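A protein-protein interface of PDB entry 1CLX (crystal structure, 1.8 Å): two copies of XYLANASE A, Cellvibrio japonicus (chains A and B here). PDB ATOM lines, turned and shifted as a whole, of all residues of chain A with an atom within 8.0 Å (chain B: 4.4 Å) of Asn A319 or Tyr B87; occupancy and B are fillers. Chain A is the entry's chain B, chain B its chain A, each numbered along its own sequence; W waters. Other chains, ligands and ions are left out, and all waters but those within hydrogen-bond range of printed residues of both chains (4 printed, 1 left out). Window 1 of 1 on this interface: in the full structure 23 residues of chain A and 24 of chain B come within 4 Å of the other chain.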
ATOM      1  N   ASN A 252      25.901  22.672   5.796  1.00  0.00           N
ATOM      2  CA  ASN A 252      25.817  23.561   4.624  1.00  0.00           C
ATOM      3  C   ASN A 252      26.215  24.997   4.965  1.00  0.00           C
ATOM      4  O   ASN A 252      25.618  25.579   5.881  1.00  0.00           O
ATOM      5  CB  ASN A 252      24.419  23.571   3.984  1.00  0.00           C
ATOM      6  CG  ASN A 252      24.204  22.313   3.137  1.00  0.00           C
ATOM      7  OD1 ASN A 252      25.202  21.913   2.363  1.00  0.00           O
ATOM      8  ND2 ASN A 252      23.102  21.605   3.142  1.00  0.00           N
ATOM      9  N   ASN A 253      27.172  25.544   4.220  1.00  0.00           N
ATOM     10  CA  ASN A 253      27.541  26.967   4.297  1.00  0.00           C
ATOM     11  C   ASN A 253      27.121  27.710   3.044  1.00  0.00           C
ATOM     12  O   ASN A 253      27.790  27.600   2.004  1.00  0.00           O
ATOM     13  CB  ASN A 253      29.052  27.103   4.513  1.00  0.00           C
ATOM     14  CG  ASN A 253      29.453  28.562   4.777  1.00  0.00           C
ATOM     15  OD1 ASN A 253      28.564  29.479   4.468  1.00  0.00           O
ATOM     16  ND2 ASN A 253      30.629  28.867   5.302  1.00  0.00           N
ATOM     17  N   PRO A 254      25.972  28.389   3.071  1.00  0.00           N
ATOM     18  CA  PRO A 254      25.589  28.972   1.758  1.00  0.00           C
ATOM     19  C   PRO A 254      26.181  30.377   1.715  1.00  0.00           C
ATOM     20  O   PRO A 254      25.750  31.144   0.863  1.00  0.00           O
ATOM     21  CB  PRO A 254      24.085  29.062   1.933  1.00  0.00           C
ATOM     22  CG  PRO A 254      23.872  29.347   3.402  1.00  0.00           C
ATOM     23  CD  PRO A 254      24.935  28.519   4.099  1.00  0.00           C
ATOM     24  N   TYR A 255      27.109  30.703   2.602  1.00  0.00           N
ATOM     25  CA  TYR A 255      27.800  31.995   2.522  1.00  0.00           C
ATOM     26  C   TYR A 255      29.239  31.902   2.095  1.00  0.00           C
ATOM     27  O   TYR A 255      29.956  32.900   2.096  1.00  0.00           O
ATOM     28  CB  TYR A 255      27.719  32.816   3.796  1.00  0.00           C
ATOM     29  CG  TYR A 255      26.293  32.765   4.337  1.00  0.00           C
ATOM     30  CD1 TYR A 255      25.247  33.324   3.612  1.00  0.00           C
ATOM     31  CD2 TYR A 255      26.063  32.151   5.562  1.00  0.00           C
ATOM     32  CE1 TYR A 255      23.952  33.259   4.117  1.00  0.00           C
ATOM     33  CE2 TYR A 255      24.769  32.096   6.058  1.00  0.00           C
ATOM     34  CZ  TYR A 255      23.709  32.643   5.341  1.00  0.00           C
ATOM     35  OH  TYR A 255      22.421  32.576   5.840  1.00  0.00           O
ATOM     36  N   ASP A 256      29.697  30.741   1.670  1.00  0.00           N
ATOM     37  CA  ASP A 256      31.136  30.661   1.373  1.00  0.00           C
ATOM     38  C   ASP A 256      31.428  30.866  -0.102  1.00  0.00           C
ATOM     39  O   ASP A 256      32.579  30.649  -0.495  1.00  0.00           O
ATOM     40  CB  ASP A 256      31.629  29.277   1.807  1.00  0.00           C
ATOM     41  CG  ASP A 256      30.846  28.201   1.058  1.00  0.00           C
ATOM     42  OD1 ASP A 256      30.022  28.471   0.168  1.00  0.00           O
ATOM     43  OD2 ASP A 256      31.046  27.022   1.349  1.00  0.00           O
ATOM     44  N   GLY A 257      30.486  31.235  -0.946  1.00  0.00           N
ATOM     45  CA  GLY A 257      30.747  31.589  -2.355  1.00  0.00           C
ATOM     46  C   GLY A 257      30.989  30.379  -3.229  1.00  0.00           C
ATOM     47  O   GLY A 257      31.494  30.472  -4.350  1.00  0.00           O
ATOM     48  N   ASN A 258      30.573  29.217  -2.753  1.00  0.00           N
ATOM     49  CA  ASN A 258      30.754  27.935  -3.448  1.00  0.00           C
ATOM     50  C   ASN A 258      29.473  27.134  -3.374  1.00  0.00           C
ATOM     51  O   ASN A 258      29.141  26.507  -2.378  1.00  0.00           O
ATOM     52  CB  ASN A 258      31.931  27.193  -2.815  1.00  0.00           C
ATOM     53  CG  ASN A 258      32.309  25.938  -3.565  1.00  0.00           C
ATOM     54  OD1 ASN A 258      31.568  25.461  -4.542  1.00  0.00           O
ATOM     55  ND2 ASN A 258      33.410  25.282  -3.226  1.00  0.00           N
ATOM     56  N   SER A 259      28.721  27.048  -4.448  1.00  0.00           N
ATOM     57  CA  SER A 259      27.496  26.234  -4.405  1.00  0.00           C
ATOM     58  C   SER A 259      27.775  24.802  -4.822  1.00  0.00           C
ATOM     59  O   SER A 259      26.846  24.005  -4.934  1.00  0.00           O
ATOM     60  CB  SER A 259      26.437  26.878  -5.286  1.00  0.00           C
ATOM     61  OG  SER A 259      27.031  27.026  -6.599  1.00  0.00           O
ATOM     62  N   SER A 260      29.031  24.419  -4.994  1.00  0.00           N
ATOM     63  CA  SER A 260      29.412  23.081  -5.426  1.00  0.00           C
ATOM     64  C   SER A 260      29.659  22.151  -4.249  1.00  0.00           C
ATOM     65  O   SER A 260      29.593  20.930  -4.415  1.00  0.00           O
ATOM     66  CB  SER A 260      30.631  23.083  -6.322  1.00  0.00           C
ATOM     67  OG  SER A 260      30.319  23.704  -7.574  1.00  0.00           O
ATOM     68  N   ASP A 262      27.666  22.204  -1.484  1.00  0.00           N
ATOM     69  CA  ASP A 262      26.419  22.101  -0.691  1.00  0.00           C
ATOM     70  C   ASP A 262      25.779  20.724  -0.810  1.00  0.00           C
ATOM     71  O   ASP A 262      25.689  20.123  -1.887  1.00  0.00           O
ATOM     72  CB  ASP A 262      25.401  23.171  -1.142  1.00  0.00           C
ATOM     73  CG  ASP A 262      25.945  24.582  -0.930  1.00  0.00           C
ATOM     74  OD1 ASP A 262      26.922  24.720  -0.172  1.00  0.00           O
ATOM     75  OD2 ASP A 262      25.438  25.573  -1.496  1.00  0.00           O
ATOM     76  N   TYR A 263      25.193  20.188   0.249  1.00  0.00           N
ATOM     77  CA  TYR A 263      24.306  19.006   0.128  1.00  0.00           C
ATOM     78  C   TYR A 263      22.906  19.510  -0.223  1.00  0.00           C
ATOM     79  O   TYR A 263      22.292  20.162   0.621  1.00  0.00           O
ATOM     80  CB  TYR A 263      24.195  18.329   1.508  1.00  0.00           C
ATOM     81  CG  TYR A 263      25.560  17.764   1.888  1.00  0.00           C
ATOM     82  CD1 TYR A 263      26.020  16.661   1.165  1.00  0.00           C
ATOM     83  CD2 TYR A 263      26.331  18.332   2.901  1.00  0.00           C
ATOM     84  CE1 TYR A 263      27.265  16.136   1.506  1.00  0.00           C
ATOM     85  CE2 TYR A 263      27.587  17.793   3.230  1.00  0.00           C
ATOM     86  CZ  TYR A 263      28.051  16.684   2.518  1.00  0.00           C
ATOM     87  OH  TYR A 263      29.284  16.106   2.779  1.00  0.00           O
ATOM     88  N   THR A 264      22.397  19.131  -1.377  1.00  0.00           N
ATOM     89  CA  THR A 264      21.108  19.699  -1.824  1.00  0.00           C
ATOM     90  C   THR A 264      19.961  18.734  -1.625  1.00  0.00           C
ATOM     91  O   THR A 264      18.789  19.077  -1.786  1.00  0.00           O
ATOM     92  CB  THR A 264      21.150  20.218  -3.248  1.00  0.00           C
ATOM     93  OG1 THR A 264      21.616  19.212  -4.144  1.00  0.00           O
ATOM     94  CG2 THR A 264      22.071  21.404  -3.339  1.00  0.00           C
ATOM     95  N   ASN A 265      20.237  17.525  -1.184  1.00  0.00           N
ATOM     96  CA  ASN A 265      19.217  16.459  -1.194  1.00  0.00           C
ATOM     97  C   ASN A 265      19.081  15.910   0.217  1.00  0.00           C
ATOM     98  O   ASN A 265      20.096  15.724   0.881  1.00  0.00           O
ATOM     99  CB  ASN A 265      19.628  15.380  -2.201  1.00  0.00           C
ATOM    100  CG  ASN A 265      18.430  14.494  -2.527  1.00  0.00           C
ATOM    101  OD1 ASN A 265      17.903  13.809  -1.532  1.00  0.00           O
ATOM    102  ND2 ASN A 265      17.907  14.398  -3.734  1.00  0.00           N
ATOM    103  N   TYR A 315      16.663  22.513  10.187  1.00  0.00           N
ATOM    104  CA  TYR A 315      16.540  21.244   9.437  1.00  0.00           C
ATOM    105  C   TYR A 315      16.432  21.549   7.942  1.00  0.00           C
ATOM    106  O   TYR A 315      16.812  20.745   7.094  1.00  0.00           O
ATOM    107  CB  TYR A 315      15.279  20.551   9.890  1.00  0.00           C
ATOM    108  CG  TYR A 315      15.163  19.102   9.402  1.00  0.00           C
ATOM    109  CD1 TYR A 315      16.139  18.133   9.625  1.00  0.00           C
ATOM    110  CD2 TYR A 315      13.988  18.782   8.731  1.00  0.00           C
ATOM    111  CE1 TYR A 315      15.974  16.814   9.170  1.00  0.00           C
ATOM    112  CE2 TYR A 315      13.804  17.489   8.271  1.00  0.00           C
ATOM    113  CZ  TYR A 315      14.787  16.520   8.499  1.00  0.00           C
ATOM    114  OH  TYR A 315      14.513  15.259   8.006  1.00  0.00           O
ATOM    115  N   THR A 316      15.899  22.729   7.709  1.00  0.00           N
ATOM    116  CA  THR A 316      15.945  23.522   6.479  1.00  0.00           C
ATOM    117  C   THR A 316      16.360  24.963   6.709  1.00  0.00           C
ATOM    118  O   THR A 316      15.898  25.638   7.626  1.00  0.00           O
ATOM    119  CB  THR A 316      14.569  23.486   5.818  1.00  0.00           C
ATOM    120  OG1 THR A 316      14.260  22.142   5.444  1.00  0.00           O
ATOM    121  CG2 THR A 316      14.570  24.343   4.590  1.00  0.00           C
ATOM    122  N   HIS A 317      17.232  25.493   5.867  1.00  0.00           N
ATOM    123  CA  HIS A 317      17.685  26.885   5.971  1.00  0.00           C
ATOM    124  C   HIS A 317      18.221  27.315   4.607  1.00  0.00           C
ATOM    125  O   HIS A 317      18.886  26.495   3.957  1.00  0.00           O
ATOM    126  CB  HIS A 317      18.728  27.102   7.062  1.00  0.00           C
ATOM    127  CG  HIS A 317      20.113  26.525   6.794  1.00  0.00           C
ATOM    128  ND1 HIS A 317      20.481  25.176   6.850  1.00  0.00           N
ATOM    129  CD2 HIS A 317      21.246  27.281   6.480  1.00  0.00           C
ATOM    130  CE1 HIS A 317      21.831  25.110   6.538  1.00  0.00           C
ATOM    131  NE2 HIS A 317      22.312  26.404   6.324  1.00  0.00           N
ATOM    132  N   GLN A 318      17.935  28.537   4.189  1.00  0.00           N
ATOM    133  CA  GLN A 318      18.363  29.009   2.858  1.00  0.00           C
ATOM    134  C   GLN A 318      17.941  27.966   1.813  1.00  0.00           C
ATOM    135  O   GLN A 318      18.729  27.726   0.888  1.00  0.00           O
ATOM    136  CB  GLN A 318      19.894  29.123   2.762  1.00  0.00           C
ATOM    137  CG  GLN A 318      20.467  30.410   3.322  1.00  0.00           C
ATOM    138  CD  GLN A 318      19.548  31.589   2.984  1.00  0.00           C
ATOM    139  OE1 GLN A 318      18.649  31.993   3.881  1.00  0.00           O
ATOM    140  NE2 GLN A 318      19.615  32.198   1.806  1.00  0.00           N
ATOM    141  N   ASN A 319      16.785  27.344   1.940  1.00  0.00           N
ATOM    142  CA  ASN A 319      16.321  26.332   0.988  1.00  0.00           C
ATOM    143  C   ASN A 319      17.193  25.109   0.808  1.00  0.00           C
ATOM    144  O   ASN A 319      17.081  24.397  -0.192  1.00  0.00           O
ATOM    145  CB  ASN A 319      15.986  26.951  -0.370  1.00  0.00           C
ATOM    146  CG  ASN A 319      14.658  27.720  -0.328  1.00  0.00           C
ATOM    147  OD1 ASN A 319      14.637  29.035  -0.171  1.00  0.00           O
ATOM    148  ND2 ASN A 319      13.520  27.053  -0.464  1.00  0.00           N
ATOM    149  N   LEU A 320      17.979  24.725   1.786  1.00  0.00           N
ATOM    150  CA  LEU A 320      18.954  23.624   1.731  1.00  0.00           C
ATOM    151  C   LEU A 320      18.646  22.663   2.921  1.00  0.00           C
ATOM    152  O   LEU A 320      18.230  23.201   3.964  1.00  0.00           O
ATOM    153  CB  LEU A 320      20.339  24.216   1.958  1.00  0.00           C
ATOM    154  CG  LEU A 320      20.997  24.845   0.747  1.00  0.00           C
ATOM    155  CD1 LEU A 320      22.403  25.290   1.138  1.00  0.00           C
ATOM    156  CD2 LEU A 320      21.083  23.959  -0.488  1.00  0.00           C
ATOM    157  N   PRO A 321      18.718  21.353   2.736  1.00  0.00           N
ATOM    158  CA  PRO A 321      18.514  20.452   3.895  1.00  0.00           C
ATOM    159  C   PRO A 321      19.707  20.576   4.831  1.00  0.00           C
ATOM    160  O   PRO A 321      20.790  21.010   4.455  1.00  0.00           O
ATOM    161  CB  PRO A 321      18.524  19.094   3.191  1.00  0.00           C
ATOM    162  CG  PRO A 321      19.550  19.254   2.070  1.00  0.00           C
ATOM    163  CD  PRO A 321      19.230  20.645   1.547  1.00  0.00           C
ATOM    164  N   ASP A 322      19.517  20.313   6.116  1.00  0.00           N
ATOM    165  CA  ASP A 322      20.658  20.288   7.025  1.00  0.00           C
ATOM    166  C   ASP A 322      20.354  19.335   8.173  1.00  0.00           C
ATOM    167  O   ASP A 322      19.228  18.852   8.305  1.00  0.00           O
ATOM    168  CB  ASP A 322      21.085  21.662   7.545  1.00  0.00           C
ATOM    169  CG  ASP A 322      22.621  21.751   7.571  1.00  0.00           C
ATOM    170  OD1 ASP A 322      23.286  20.880   8.157  1.00  0.00           O
ATOM    171  OD2 ASP A 322      23.229  22.679   7.034  1.00  0.00           O
ATOM    172  N   ASN B  44      12.883  24.588  -6.245  1.00  0.00           N
ATOM    173  CA  ASN B  44      14.302  24.846  -6.144  1.00  0.00           C
ATOM    174  C   ASN B  44      15.195  24.453  -7.298  1.00  0.00           C
ATOM    175  O   ASN B  44      16.262  25.056  -7.437  1.00  0.00           O
ATOM    176  CB  ASN B  44      14.930  24.179  -4.898  1.00  0.00           C
ATOM    177  CG  ASN B  44      14.711  25.178  -3.760  1.00  0.00           C
ATOM    178  OD1 ASN B  44      15.482  26.237  -3.688  1.00  0.00           O
ATOM    179  ND2 ASN B  44      13.743  24.906  -2.922  1.00  0.00           N
ATOM    180  N   LYS B  47      16.710  26.801 -10.065  1.00  0.00           N
ATOM    181  CA  LYS B  47      17.528  27.928  -9.600  1.00  0.00           C
ATOM    182  C   LYS B  47      18.931  27.926 -10.173  1.00  0.00           C
ATOM    183  O   LYS B  47      19.372  26.908 -10.724  1.00  0.00           O
ATOM    184  CB  LYS B  47      17.547  27.936  -8.079  1.00  0.00           C
ATOM    185  CG  LYS B  47      16.158  28.341  -7.598  1.00  0.00           C
ATOM    186  CD  LYS B  47      16.089  28.339  -6.081  1.00  0.00           C
ATOM    187  CE  LYS B  47      14.697  28.843  -5.718  1.00  0.00           C
ATOM    188  NZ  LYS B  47      14.321  28.505  -4.339  1.00  0.00           N
ATOM    189  N   SER B  49      22.407  27.828  -9.655  1.00  0.00           N
ATOM    190  CA  SER B  49      23.487  26.869  -9.381  1.00  0.00           C
ATOM    191  C   SER B  49      23.152  25.440  -9.786  1.00  0.00           C
ATOM    192  O   SER B  49      24.036  24.614 -10.001  1.00  0.00           O
ATOM    193  CB  SER B  49      23.817  26.924  -7.897  1.00  0.00           C
ATOM    194  OG  SER B  49      22.644  26.665  -7.102  1.00  0.00           O
ATOM    195  N   TRP B  83      18.754  35.520 -10.414  1.00  0.00           N
ATOM    196  CA  TRP B  83      18.269  35.805  -9.052  1.00  0.00           C
ATOM    197  C   TRP B  83      19.447  35.843  -8.083  1.00  0.00           C
ATOM    198  O   TRP B  83      20.435  35.141  -8.323  1.00  0.00           O
ATOM    199  CB  TRP B  83      17.313  34.666  -8.721  1.00  0.00           C
ATOM    200  CG  TRP B  83      16.535  34.988  -7.455  1.00  0.00           C
ATOM    201  CD1 TRP B  83      16.098  36.185  -7.053  1.00  0.00           C
ATOM    202  CD2 TRP B  83      16.183  34.033  -6.493  1.00  0.00           C
ATOM    203  NE1 TRP B  83      15.445  35.989  -5.795  1.00  0.00           N
ATOM    204  CE2 TRP B  83      15.495  34.715  -5.481  1.00  0.00           C
ATOM    205  CE3 TRP B  83      16.376  32.655  -6.361  1.00  0.00           C
ATOM    206  CZ2 TRP B  83      15.011  34.075  -4.385  1.00  0.00           C
ATOM    207  CZ3 TRP B  83      15.873  32.002  -5.233  1.00  0.00           C
ATOM    208  CH2 TRP B  83      15.189  32.705  -4.239  1.00  0.00           C
ATOM    209  N   PRO B  85      20.204  35.294  -4.498  1.00  0.00           N
ATOM    210  CA  PRO B  85      20.601  34.757  -3.185  1.00  0.00           C
ATOM    211  C   PRO B  85      21.801  33.832  -3.283  1.00  0.00           C
ATOM    212  O   PRO B  85      21.902  32.956  -4.132  1.00  0.00           O
ATOM    213  CB  PRO B  85      19.373  33.978  -2.768  1.00  0.00           C
ATOM    214  CG  PRO B  85      18.215  34.734  -3.393  1.00  0.00           C
ATOM    215  CD  PRO B  85      18.766  35.191  -4.742  1.00  0.00           C
ATOM    216  N   SER B  86      22.742  34.055  -2.386  1.00  0.00           N
ATOM    217  CA  SER B  86      24.079  33.461  -2.515  1.00  0.00           C
ATOM    218  C   SER B  86      23.977  31.955  -2.588  1.00  0.00           C
ATOM    219  O   SER B  86      24.787  31.312  -3.260  1.00  0.00           O
ATOM    220  CB  SER B  86      24.995  33.928  -1.403  1.00  0.00           C
ATOM    221  OG  SER B  86      24.446  33.514  -0.132  1.00  0.00           O
ATOM    222  N   TYR B  87      23.007  31.335  -1.929  1.00  0.00           N
ATOM    223  CA  TYR B  87      23.036  29.868  -1.895  1.00  0.00           C
ATOM    224  C   TYR B  87      22.850  29.266  -3.270  1.00  0.00           C
ATOM    225  O   TYR B  87      23.196  28.102  -3.501  1.00  0.00           O
ATOM    226  CB  TYR B  87      22.044  29.272  -0.926  1.00  0.00           C
ATOM    227  CG  TYR B  87      20.606  29.477  -1.389  1.00  0.00           C
ATOM    228  CD1 TYR B  87      19.915  30.643  -1.117  1.00  0.00           C
ATOM    229  CD2 TYR B  87      19.975  28.442  -2.092  1.00  0.00           C
ATOM    230  CE1 TYR B  87      18.589  30.810  -1.519  1.00  0.00           C
ATOM    231  CE2 TYR B  87      18.655  28.616  -2.504  1.00  0.00           C
ATOM    232  CZ  TYR B  87      17.963  29.782  -2.222  1.00  0.00           C
ATOM    233  OH  TYR B  87      16.646  29.886  -2.653  1.00  0.00           O
ATOM    234  N   GLN B  88      22.183  29.995  -4.154  1.00  0.00           N
ATOM    235  CA  GLN B  88      21.956  29.478  -5.510  1.00  0.00           C
ATOM    236  C   GLN B  88      22.775  30.190  -6.565  1.00  0.00           C
ATOM    237  O   GLN B  88      22.520  30.022  -7.759  1.00  0.00           O
ATOM    238  CB  GLN B  88      20.479  29.388  -5.865  1.00  0.00           C
ATOM    239  CG  GLN B  88      19.770  30.727  -5.643  1.00  0.00           C
ATOM    240  CD  GLN B  88      19.949  31.605  -6.868  1.00  0.00           C
ATOM    241  OE1 GLN B  88      20.655  32.725  -6.816  1.00  0.00           O
ATOM    242  NE2 GLN B  88      19.392  31.230  -8.014  1.00  0.00           N
ATOM    243  N   LEU B  89      23.786  30.971  -6.216  1.00  0.00           N
ATOM    244  CA  LEU B  89      24.591  31.671  -7.237  1.00  0.00           C
ATOM    245  C   LEU B  89      25.541  30.670  -7.894  1.00  0.00           C
ATOM    246  O   LEU B  89      26.189  29.958  -7.122  1.00  0.00           O
ATOM    247  CB  LEU B  89      25.367  32.813  -6.613  1.00  0.00           C
ATOM    248  CG  LEU B  89      24.567  34.102  -6.483  1.00  0.00           C
ATOM    249  CD1 LEU B  89      25.391  35.264  -5.957  1.00  0.00           C
ATOM    250  CD2 LEU B  89      23.824  34.526  -7.730  1.00  0.00           C
HETATM  251  O   HOH W   1      28.422  30.618  -5.466  1.00  0.00           O
HETATM  252  O   HOH W   2      23.192  25.461  -3.562  1.00  0.00           O
HETATM  253  O   HOH W   3      27.127  29.420  -2.882  1.00  0.00           O
HETATM  254  O   HOH W   4      22.002  32.333   0.736  1.00  0.00           O
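O of Leu B89 is in hydrogen-bond range of OG of Ser A259 (3.1 Å). The side-chain hydroxyl (OH) of Tyr B87 lies within hydrogen-bond range of the side-chain amide oxygen (OD1) of Asn A319 (3.3 Å). The side-chain amide nitrogen (ND2) of Asn B44 sits close to the side-chain amide nitrogen (ND2) of Asn A319. The side-chain hydroxyl (OG) of Ser B86 lies within hydrogen-bond range of the backbone carbonyl oxygen (O) of Pro A254 (2.9 Å).
The side-chain amide oxygen of Asn B44 sits at hydrogen-bond distance from the side-chain amino group of Lys B47 (2.6 Å). The side-chain hydroxyl (OH) of Tyr B87 sits at hydrogen-bond distance from the side-chain amino group (NZ) of Lys B47, at 3.2 Å. N of Ser B49 sits at hydrogen-bond distance from O of Gln B88 (2.9 Å). The side-chain amide oxygen (OD1) of Asn A253 sits at hydrogen-bond distance from the backbone NH (N) of Tyr A255.
Among the printed residues, merely in contact across the chains: Pro A254 with Tyr B87 (3.5 Å), Tyr A255 with Ser B86 (3.8 Å), Ser A259 with Ser B49 (3.5 Å), Ser A259 with Tyr B87 (3.9 Å), Asp A262 with Tyr B87 (3.9 Å) and Gln A318 with Tyr B87 (3.3 Å).
Of chain B, only Asn B44 and Tyr B87 come within 4 Å of Asn A319. Of the printed residues of chain A, Tyr B87 touches Pro A254 (3.5 Å), Ser A259 (3.9 Å), Asp A262 (3.9 Å), Gln A318 (3.3 Å) and Asn A319 (3.3 Å). Of the printed residues of chain B, Ser A259 touches Ser B49, Tyr B87 and Leu B89. Of the printed residues of chain A, Ser B49 touches Ser A259 (3.5 Å). Printed residues of chain B within 4 Å of Tyr A255: Ser B86 (3.8 Å). Asp A322 touches none of the printed residues of chain B. Asn A253 touches none of the printed residues of chain B. The nearest residue of chain B that does not touch Asn A319 is Lys B47 (4.1 Å). The nearest residue of chain A that does not touch Tyr B87 is Leu A320 (4.5 Å). The nearest printed residue of chain A that does not touch Leu B89 is Asn A258 (5.7 Å).
Of the 9 printed residues of chain B, 5 touch a printed residue of chain A. Printed residues of chain B that touch a printed residue of chain A: Asn B44, Ser B49, Ser B86, Tyr B87 and Leu B89. Hydrophobic or aromatic side chains of chain B that line the printed part of chain A: Tyr B87. Of the 21 printed residues of chain A, 6 touch a printed residue of chain B. Among the printed residues, 10 pairs touch across the chains.
No position is printed for both chains.
Water W4 lies within hydrogen-bond range of the side-chain amide nitrogen of Gln A318 (2.6 Å), the side-chain hydroxyl of Ser B86 (2.8 Å) and the backbone NH of Tyr B87 (3.0 Å). Water W2 lies within hydrogen-bond range of O of Tyr B87 and OD2 of Asp A262. Water W1 bridges the backbone carbonyl oxygen (O) of Leu B89 (2.9 Å) and the backbone carbonyl oxygen (O) of Gly A257 (3.3 Å). Water W3 lies within hydrogen-bond range of O of Ser B86 (3.0 Å), N of Ser A259 (3.3 Å) and N of Asn A258 (3.5 Å).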
